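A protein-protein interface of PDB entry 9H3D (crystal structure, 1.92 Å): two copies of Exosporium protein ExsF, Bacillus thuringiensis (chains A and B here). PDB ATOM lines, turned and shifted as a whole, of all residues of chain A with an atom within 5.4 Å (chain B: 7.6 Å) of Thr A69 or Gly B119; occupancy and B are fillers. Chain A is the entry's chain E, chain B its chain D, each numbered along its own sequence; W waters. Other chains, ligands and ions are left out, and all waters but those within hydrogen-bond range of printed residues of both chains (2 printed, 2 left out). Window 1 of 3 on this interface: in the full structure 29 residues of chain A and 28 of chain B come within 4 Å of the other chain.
Ser A117 touches its own counterpart, Ser B117. Ser A117 touches Ser B118, but with the chains exchanged Ser A118 does not touch Ser B117 (6.7 Å). Of the 11 pairs that touch across the chains among the printed residues, 1 has its exchanged pair printed and touching as well.
OH of Tyr B68 is in hydrogen-bond range of OG1 of Thr B102 (2.9 Å). The backbone NH (N) of Ser B118 is in hydrogen-bond range of the backbone carbonyl oxygen (O) of Tyr B68. The backbone NH (N) of Thr A150 sits at hydrogen-bond distance from the backbone carbonyl oxygen (O) of Ser A67, at 2.9 Å. O of Val A116 is in hydrogen-bond range of OG1 of Thr A69 (3.3 Å). The backbone NH (N) of Thr A69 is in hydrogen-bond range of the backbone carbonyl oxygen (O) of Ala A148 (3.1 Å). N of Thr A71 sits at hydrogen-bond distance from O of Ala A146, 2.9 Å away.
Thr A69 touches just these residues of chain B: Ser B117 (3.5 Å) and Gly B119 (3.5 Å). Gly B119 touches just one residue of chain A: Thr A69. Printed residues of chain A within 4 Å of Val B120: Ser A67 and Thr A150. Of the printed residues of chain A, Ser B118 touches Ser A117. Of the printed residues of chain B, Ser A117 touches Ser B117 (2.8 Å) and Ser B118 (3.6 Å). Ala A146 touches none of the printed residues of chain B. Tyr A68 touches none of the printed residues of chain B. The nearest residue of chain A that does not touch Gly B119 is Ser A117 (4.8 Å). The nearest printed residue of chain A that does not touch Val B120 is Thr A69 (5.7 Å).
Water W2 bridges OG of Ser A67 (2.7 Å) and N of Val B120 (2.9 Å). Water W1 lies within hydrogen-bond range of the side-chain hydroxyl (OG1) of Thr A69 (2.8 Å), the side-chain hydroxyl (OG1) of Thr A71 (2.9 Å) and the backbone carbonyl oxygen (O) of Gly B101 (3.3 Å).
Val B120 touches Ser A67. Ser B117 touches Thr A69 (O to OG1, 3.5 Å). CG2 of Thr A69 touches N of Gly B119 (3.5 Å). Thr B102 touches Thr A71. Asp A115 touches Thr B102 (OD1 to CG2, 3.6 Å). Val B116 touches Asp A115. Ser A117 touches Ser B118 (OG to O, 3.6 Å). Leu B122 touches Thr A150 (CD2 to CG2, 3.8 Å).
The backbone NH (N) of Ser B117 sits at hydrogen-bond distance from the side-chain carboxylate (OD2) of Asp A115. The side-chain hydroxyl of Ser A117 lies within hydrogen-bond range of the backbone carbonyl oxygen of Ser B117. The backbone carbonyl oxygen (O) of Val B120 sits at hydrogen-bond distance from the side-chain hydroxyl (OG1) of Thr A150 (2.6 Å).
Of the 16 printed residues of chain B, 7 touch a printed residue of chain A. Printed residues of chain B that touch a printed residue of chain A: Thr B102, Val B116, Ser B117, Ser B118, Gly B119, Val B120 and Leu B122. Hydrophobic or aromatic side chains of chain B that line the printed part of chain A: Val B120 and Leu B122.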
ATOM      1  N   SER A  67      32.717 -13.265  19.255  1.00  0.00           N
ATOM      2  CA  SER A  67      31.271 -13.451  19.277  1.00  0.00           C
ATOM      3  C   SER A  67      30.716 -13.099  17.905  1.00  0.00           C
ATOM      4  O   SER A  67      31.401 -12.497  17.072  1.00  0.00           O
ATOM      5  CB  SER A  67      30.621 -12.611  20.380  1.00  0.00           C
ATOM      6  OG  SER A  67      30.832 -11.225  20.167  1.00  0.00           O
ATOM      7  N   TYR A  68      29.462 -13.477  17.680  1.00  0.00           N
ATOM      8  CA  TYR A  68      28.792 -13.148  16.429  1.00  0.00           C
ATOM      9  C   TYR A  68      27.296 -12.924  16.652  1.00  0.00           C
ATOM     10  O   TYR A  68      26.699 -13.411  17.621  1.00  0.00           O
ATOM     11  CB  TYR A  68      29.015 -14.232  15.368  1.00  0.00           C
ATOM     12  CG  TYR A  68      28.476 -15.618  15.721  1.00  0.00           C
ATOM     13  CD1 TYR A  68      27.159 -15.971  15.443  1.00  0.00           C
ATOM     14  CD2 TYR A  68      29.305 -16.576  16.296  1.00  0.00           C
ATOM     15  CE1 TYR A  68      26.671 -17.242  15.759  1.00  0.00           C
ATOM     16  CE2 TYR A  68      28.836 -17.856  16.604  1.00  0.00           C
ATOM     17  CZ  TYR A  68      27.514 -18.180  16.336  1.00  0.00           C
ATOM     18  OH  TYR A  68      27.047 -19.448  16.659  1.00  0.00           O
ATOM     19  N   THR A  69      26.697 -12.184  15.718  1.00  0.00           N
ATOM     20  CA  THR A  69      25.256 -12.008  15.618  1.00  0.00           C
ATOM     21  C   THR A  69      24.832 -12.440  14.224  1.00  0.00           C
ATOM     22  O   THR A  69      25.587 -12.269  13.261  1.00  0.00           O
ATOM     23  CB  THR A  69      24.846 -10.530  15.860  1.00  0.00           C
ATOM     24  OG1 THR A  69      23.424 -10.368  15.713  1.00  0.00           O
ATOM     25  CG2 THR A  69      25.541  -9.600  14.856  1.00  0.00           C
ATOM     26  N   LEU A  70      23.641 -13.028  14.120  1.00  0.00           N
ATOM     27  CA  LEU A  70      23.013 -13.336  12.842  1.00  0.00           C
ATOM     28  C   LEU A  70      21.566 -12.855  12.838  1.00  0.00           C
ATOM     29  O   LEU A  70      20.835 -13.026  13.820  1.00  0.00           O
ATOM     30  CB  LEU A  70      23.028 -14.840  12.534  1.00  0.00           C
ATOM     31  CG  LEU A  70      24.371 -15.532  12.730  1.00  0.00           C
ATOM     32  CD1 LEU A  70      24.178 -17.053  12.698  1.00  0.00           C
ATOM     33  CD2 LEU A  70      25.365 -15.060  11.667  1.00  0.00           C
ATOM     34  N   THR A  71      21.136 -12.302  11.709  1.00  0.00           N
ATOM     35  CA  THR A  71      19.717 -12.108  11.435  1.00  0.00           C
ATOM     36  C   THR A  71      19.319 -13.081  10.337  1.00  0.00           C
ATOM     37  O   THR A  71      19.845 -13.006   9.214  1.00  0.00           O
ATOM     38  CB  THR A  71      19.393 -10.667  11.035  1.00  0.00           C
ATOM     39  OG1 THR A  71      19.812  -9.795  12.081  1.00  0.00           O
ATOM     40  CG2 THR A  71      17.879 -10.524  10.857  1.00  0.00           C
ATOM     41  N   ASP A 115      16.422 -13.599  15.534  1.00  0.00           N
ATOM     42  CA  ASP A 115      17.730 -13.120  15.941  1.00  0.00           C
ATOM     43  C   ASP A 115      18.554 -14.220  16.594  1.00  0.00           C
ATOM     44  O   ASP A 115      18.034 -15.008  17.388  1.00  0.00           O
ATOM     45  CB  ASP A 115      17.631 -11.971  16.924  1.00  0.00           C
ATOM     46  CG  ASP A 115      18.977 -11.435  17.264  1.00  0.00           C
ATOM     47  OD1 ASP A 115      19.548 -10.725  16.402  1.00  0.00           O
ATOM     48  OD2 ASP A 115      19.498 -11.756  18.351  1.00  0.00           O
ATOM     49  N   VAL A 116      19.850 -14.244  16.277  1.00  0.00           N
ATOM     50  CA  VAL A 116      20.811 -15.086  16.974  1.00  0.00           C
ATOM     51  C   VAL A 116      21.968 -14.203  17.440  1.00  0.00           C
ATOM     52  O   VAL A 116      22.379 -13.277  16.731  1.00  0.00           O
ATOM     53  CB  VAL A 116      21.318 -16.228  16.066  1.00  0.00           C
ATOM     54  CG1 VAL A 116      22.450 -16.973  16.733  1.00  0.00           C
ATOM     55  CG2 VAL A 116      20.197 -17.177  15.701  1.00  0.00           C
ATOM     56  N   SER A 117      22.455 -14.446  18.653  1.00  0.00           N
ATOM     57  CA  SER A 117      23.782 -13.973  19.040  1.00  0.00           C
ATOM     58  C   SER A 117      24.484 -15.101  19.788  1.00  0.00           C
ATOM     59  O   SER A 117      23.872 -15.763  20.626  1.00  0.00           O
ATOM     60  CB  SER A 117      23.723 -12.706  19.910  1.00  0.00           C
ATOM     61  OG  SER A 117      23.210 -11.586  19.174  1.00  0.00           O
ATOM     62  N   SER A 118      25.756 -15.333  19.478  1.00  0.00           N
ATOM     63  CA  SER A 118      26.535 -16.292  20.245  1.00  0.00           C
ATOM     64  C   SER A 118      26.747 -15.751  21.653  1.00  0.00           C
ATOM     65  O   SER A 118      26.462 -14.585  21.946  1.00  0.00           O
ATOM     66  CB  SER A 118      27.888 -16.544  19.577  1.00  0.00           C
ATOM     67  OG  SER A 118      28.743 -15.399  19.718  1.00  0.00           O
ATOM     68  N   ILE A 133      32.557 -17.619  10.949  1.00  0.00           N
ATOM     69  CA  ILE A 133      31.212 -18.086  11.302  1.00  0.00           C
ATOM     70  C   ILE A 133      30.762 -19.104  10.260  1.00  0.00           C
ATOM     71  O   ILE A 133      30.609 -18.763   9.078  1.00  0.00           O
ATOM     72  CB  ILE A 133      30.193 -16.935  11.377  1.00  0.00           C
ATOM     73  CG1 ILE A 133      30.704 -15.746  12.198  1.00  0.00           C
ATOM     74  CG2 ILE A 133      28.885 -17.438  11.985  1.00  0.00           C
ATOM     75  CD1 ILE A 133      29.841 -14.477  11.990  1.00  0.00           C
ATOM     76  N   ALA A 146      21.808 -10.596   7.711  1.00  0.00           N
ATOM     77  CA  ALA A 146      22.946  -9.798   8.167  1.00  0.00           C
ATOM     78  C   ALA A 146      23.702 -10.618   9.200  1.00  0.00           C
ATOM     79  O   ALA A 146      23.149 -11.551   9.791  1.00  0.00           O
ATOM     80  CB  ALA A 146      22.513  -8.452   8.764  1.00  0.00           C
ATOM     81  N   ALA A 147      24.974 -10.268   9.392  1.00  0.00           N
ATOM     82  CA  ALA A 147      25.877 -10.978  10.293  1.00  0.00           C
ATOM     83  C   ALA A 147      27.037 -10.068  10.682  1.00  0.00           C
ATOM     84  O   ALA A 147      27.399  -9.143   9.942  1.00  0.00           O
ATOM     85  CB  ALA A 147      26.410 -12.262   9.649  1.00  0.00           C
ATOM     86  N   ALA A 148      27.613 -10.327  11.858  1.00  0.00           N
ATOM     87  CA  ALA A 148      28.748  -9.540  12.319  1.00  0.00           C
ATOM     88  C   ALA A 148      29.618 -10.419  13.202  1.00  0.00           C
ATOM     89  O   ALA A 148      29.096 -11.194  14.014  1.00  0.00           O
ATOM     90  CB  ALA A 148      28.323  -8.287  13.089  1.00  0.00           C
ATOM     91  N   LEU A 149      30.937 -10.303  13.024  1.00  0.00           N
ATOM     92  CA  LEU A 149      31.924 -11.018  13.820  1.00  0.00           C
ATOM     93  C   LEU A 149      32.740 -10.027  14.636  1.00  0.00           C
ATOM     94  O   LEU A 149      33.266  -9.049  14.088  1.00  0.00           O
ATOM     95  CB  LEU A 149      32.860 -11.834  12.926  1.00  0.00           C
ATOM     96  CG  LEU A 149      33.988 -12.586  13.635  1.00  0.00           C
ATOM     97  CD1 LEU A 149      33.433 -13.671  14.576  1.00  0.00           C
ATOM     98  CD2 LEU A 149      34.914 -13.209  12.599  1.00  0.00           C
ATOM     99  N   THR A 150      32.883 -10.300  15.929  1.00  0.00           N
ATOM    100  CA  THR A 150      33.619  -9.423  16.831  1.00  0.00           C
ATOM    101  C   THR A 150      34.785 -10.168  17.472  1.00  0.00           C
ATOM    102  O   THR A 150      34.618 -11.275  17.993  1.00  0.00           O
ATOM    103  CB  THR A 150      32.702  -8.861  17.905  1.00  0.00           C
ATOM    104  OG1 THR A 150      31.586  -8.214  17.280  1.00  0.00           O
ATOM    105  CG2 THR A 150      33.458  -7.855  18.803  1.00  0.00           C
ATOM    106  N   GLN B  65      33.130  -0.869  22.613  1.00  0.00           N
ATOM    107  CA  GLN B  65      32.150  -1.891  22.287  1.00  0.00           C
ATOM    108  C   GLN B  65      30.791  -1.342  22.696  1.00  0.00           C
ATOM    109  O   GLN B  65      30.631  -0.845  23.817  1.00  0.00           O
ATOM    110  CB  GLN B  65      32.452  -3.229  22.976  1.00  0.00           C
ATOM    111  CG  GLN B  65      32.474  -3.210  24.503  1.00  0.00           C
ATOM    112  CD  GLN B  65      32.337  -4.612  25.076  1.00  0.00           C
ATOM    113  OE1 GLN B  65      33.294  -5.177  25.607  1.00  0.00           O
ATOM    114  NE2 GLN B  65      31.145  -5.194  24.944  1.00  0.00           N
ATOM    115  N   ILE B  66      29.846  -1.340  21.759  1.00  0.00           N
ATOM    116  CA  ILE B  66      28.477  -0.930  22.046  1.00  0.00           C
ATOM    117  C   ILE B  66      27.534  -2.028  21.571  1.00  0.00           C
ATOM    118  O   ILE B  66      27.771  -2.668  20.537  1.00  0.00           O
ATOM    119  CB  ILE B  66      28.131   0.443  21.416  1.00  0.00           C
ATOM    120  CG1 ILE B  66      28.047   0.377  19.891  1.00  0.00           C
ATOM    121  CG2 ILE B  66      29.149   1.513  21.819  1.00  0.00           C
ATOM    122  CD1 ILE B  66      27.747   1.720  19.256  1.00  0.00           C
ATOM    123  N   SER B  67      26.469  -2.271  22.341  1.00  0.00           N
ATOM    124  CA  SER B  67      25.557  -3.346  21.990  1.00  0.00           C
ATOM    125  C   SER B  67      24.257  -3.163  22.757  1.00  0.00           C
ATOM    126  O   SER B  67      24.163  -2.362  23.692  1.00  0.00           O
ATOM    127  CB  SER B  67      26.165  -4.726  22.279  1.00  0.00           C
ATOM    128  OG  SER B  67      26.455  -4.851  23.665  1.00  0.00           O
ATOM    129  N   TYR B  68      23.247  -3.912  22.341  1.00  0.00           N
ATOM    130  CA  TYR B  68      21.958  -3.841  23.013  1.00  0.00           C
ATOM    131  C   TYR B  68      21.278  -5.202  23.026  1.00  0.00           C
ATOM    132  O   TYR B  68      21.617  -6.104  22.258  1.00  0.00           O
ATOM    133  CB  TYR B  68      21.017  -2.806  22.377  1.00  0.00           C
ATOM    134  CG  TYR B  68      20.659  -3.041  20.920  1.00  0.00           C
ATOM    135  CD1 TYR B  68      21.451  -2.526  19.909  1.00  0.00           C
ATOM    136  CD2 TYR B  68      19.523  -3.749  20.556  1.00  0.00           C
ATOM    137  CE1 TYR B  68      21.134  -2.711  18.565  1.00  0.00           C
ATOM    138  CE2 TYR B  68      19.209  -3.962  19.190  1.00  0.00           C
ATOM    139  CZ  TYR B  68      20.031  -3.422  18.209  1.00  0.00           C
ATOM    140  OH  TYR B  68      19.762  -3.569  16.863  1.00  0.00           O
ATOM    141  N   LEU B  88      21.395   0.707  16.408  1.00  0.00           N
ATOM    142  CA  LEU B  88      21.936   1.777  17.224  1.00  0.00           C
ATOM    143  C   LEU B  88      22.118   3.021  16.363  1.00  0.00           C
ATOM    144  O   LEU B  88      22.487   2.925  15.192  1.00  0.00           O
ATOM    145  CB  LEU B  88      23.273   1.380  17.834  1.00  0.00           C
ATOM    146  CG  LEU B  88      23.170   0.308  18.899  1.00  0.00           C
ATOM    147  CD1 LEU B  88      24.588  -0.098  19.293  1.00  0.00           C
ATOM    148  CD2 LEU B  88      22.397   0.853  20.087  1.00  0.00           C
ATOM    149  N   GLY B  99      25.919  -2.469  10.744  1.00  0.00           N
ATOM    150  CA  GLY B  99      26.447  -3.520  11.583  1.00  0.00           C
ATOM    151  C   GLY B  99      25.744  -3.672  12.923  1.00  0.00           C
ATOM    152  O   GLY B  99      25.913  -4.707  13.582  1.00  0.00           O
ATOM    153  N   SER B 100      24.978  -2.672  13.346  1.00  0.00           N
ATOM    154  CA  SER B 100      24.226  -2.743  14.591  1.00  0.00           C
ATOM    155  C   SER B 100      22.786  -3.198  14.386  1.00  0.00           C
ATOM    156  O   SER B 100      22.007  -3.205  15.344  1.00  0.00           O
ATOM    157  CB  SER B 100      24.232  -1.380  15.284  1.00  0.00           C
ATOM    158  OG  SER B 100      23.417  -0.453  14.591  1.00  0.00           O
ATOM    159  N   GLY B 101      22.422  -3.574  13.165  1.00  0.00           N
ATOM    160  CA  GLY B 101      21.047  -3.849  12.863  1.00  0.00           C
ATOM    161  C   GLY B 101      20.601  -5.226  13.319  1.00  0.00           C
ATOM    162  O   GLY B 101      21.358  -6.195  13.334  1.00  0.00           O
ATOM    163  N   THR B 102      19.333  -5.291  13.709  1.00  0.00           N
ATOM    164  CA  THR B 102      18.661  -6.546  13.994  1.00  0.00           C
ATOM    165  C   THR B 102      17.259  -6.484  13.422  1.00  0.00           C
ATOM    166  O   THR B 102      16.710  -5.408  13.167  1.00  0.00           O
ATOM    167  CB  THR B 102      18.547  -6.827  15.497  1.00  0.00           C
ATOM    168  OG1 THR B 102      17.977  -5.685  16.149  1.00  0.00           O
ATOM    169  CG2 THR B 102      19.907  -7.166  16.099  1.00  0.00           C
ATOM    170  N   VAL B 116      16.147 -10.567  21.065  1.00  0.00           N
ATOM    171  CA  VAL B 116      17.067  -9.899  20.148  1.00  0.00           C
ATOM    172  C   VAL B 116      18.311  -9.510  20.929  1.00  0.00           C
ATOM    173  O   VAL B 116      18.212  -9.054  22.078  1.00  0.00           O
ATOM    174  CB  VAL B 116      16.423  -8.644  19.516  1.00  0.00           C
ATOM    175  CG1 VAL B 116      17.473  -7.795  18.753  1.00  0.00           C
ATOM    176  CG2 VAL B 116      15.269  -9.025  18.600  1.00  0.00           C
ATOM    177  N   SER B 117      19.486  -9.694  20.310  1.00  0.00           N
ATOM    178  CA  SER B 117      20.707  -9.044  20.773  1.00  0.00           C
ATOM    179  C   SER B 117      21.506  -8.593  19.562  1.00  0.00           C
ATOM    180  O   SER B 117      21.645  -9.350  18.595  1.00  0.00           O
ATOM    181  CB  SER B 117      21.581  -9.966  21.635  1.00  0.00           C
ATOM    182  OG  SER B 117      21.066 -10.070  22.946  1.00  0.00           O
ATOM    183  N   SER B 118      22.028  -7.371  19.614  1.00  0.00           N
ATOM    184  CA  SER B 118      22.907  -6.932  18.544  1.00  0.00           C
ATOM    185  C   SER B 118      24.247  -7.636  18.660  1.00  0.00           C
ATOM    186  O   SER B 118      24.557  -8.272  19.664  1.00  0.00           O
ATOM    187  CB  SER B 118      23.151  -5.433  18.621  1.00  0.00           C
ATOM    188  OG  SER B 118      23.996  -5.147  19.733  1.00  0.00           O
ATOM    189  N   GLY B 119      25.078  -7.460  17.650  1.00  0.00           N
ATOM    190  CA  GLY B 119      26.466  -7.818  17.809  1.00  0.00           C
ATOM    191  C   GLY B 119      27.146  -6.950  18.845  1.00  0.00           C
ATOM    192  O   GLY B 119      26.629  -5.929  19.294  1.00  0.00           O
ATOM    193  N   VAL B 120      28.343  -7.374  19.245  1.00  0.00           N
ATOM    194  CA  VAL B 120      29.223  -6.518  20.033  1.00  0.00           C
ATOM    195  C   VAL B 120      29.938  -5.610  19.035  1.00  0.00           C
ATOM    196  O   VAL B 120      30.926  -6.003  18.418  1.00  0.00           O
ATOM    197  CB  VAL B 120      30.203  -7.328  20.880  1.00  0.00           C
ATOM    198  CG1 VAL B 120      31.102  -6.403  21.680  1.00  0.00           C
ATOM    199  CG2 VAL B 120      29.443  -8.254  21.823  1.00  0.00           C
ATOM    200  N   ILE B 121      29.429  -4.402  18.848  1.00  0.00           N
ATOM    201  CA  ILE B 121      29.876  -3.539  17.764  1.00  0.00           C
ATOM    202  C   ILE B 121      31.092  -2.754  18.247  1.00  0.00           C
ATOM    203  O   ILE B 121      31.035  -2.080  19.277  1.00  0.00           O
ATOM    204  CB  ILE B 121      28.740  -2.604  17.324  1.00  0.00           C
ATOM    205  CG1 ILE B 121      27.494  -3.435  16.989  1.00  0.00           C
ATOM    206  CG2 ILE B 121      29.175  -1.680  16.160  1.00  0.00           C
ATOM    207  CD1 ILE B 121      26.307  -2.862  17.607  1.00  0.00           C
ATOM    208  N   LEU B 122      32.207  -2.861  17.536  1.00  0.00           N
ATOM    209  CA  LEU B 122      33.395  -2.092  17.884  1.00  0.00           C
ATOM    210  C   LEU B 122      33.413  -0.868  16.986  1.00  0.00           C
ATOM    211  O   LEU B 122      33.208  -0.990  15.770  1.00  0.00           O
ATOM    212  CB  LEU B 122      34.680  -2.917  17.707  1.00  0.00           C
ATOM    213  CG  LEU B 122      34.760  -4.322  18.321  1.00  0.00           C
ATOM    214  CD1 LEU B 122      36.217  -4.866  18.281  1.00  0.00           C
ATOM    215  CD2 LEU B 122      34.232  -4.303  19.747  1.00  0.00           C
HETATM  216  O   HOH W   1      22.430  -9.281  13.304  1.00  0.00           O
HETATM  217  O   HOH W   2      28.729 -10.174  18.836  1.00  0.00           O
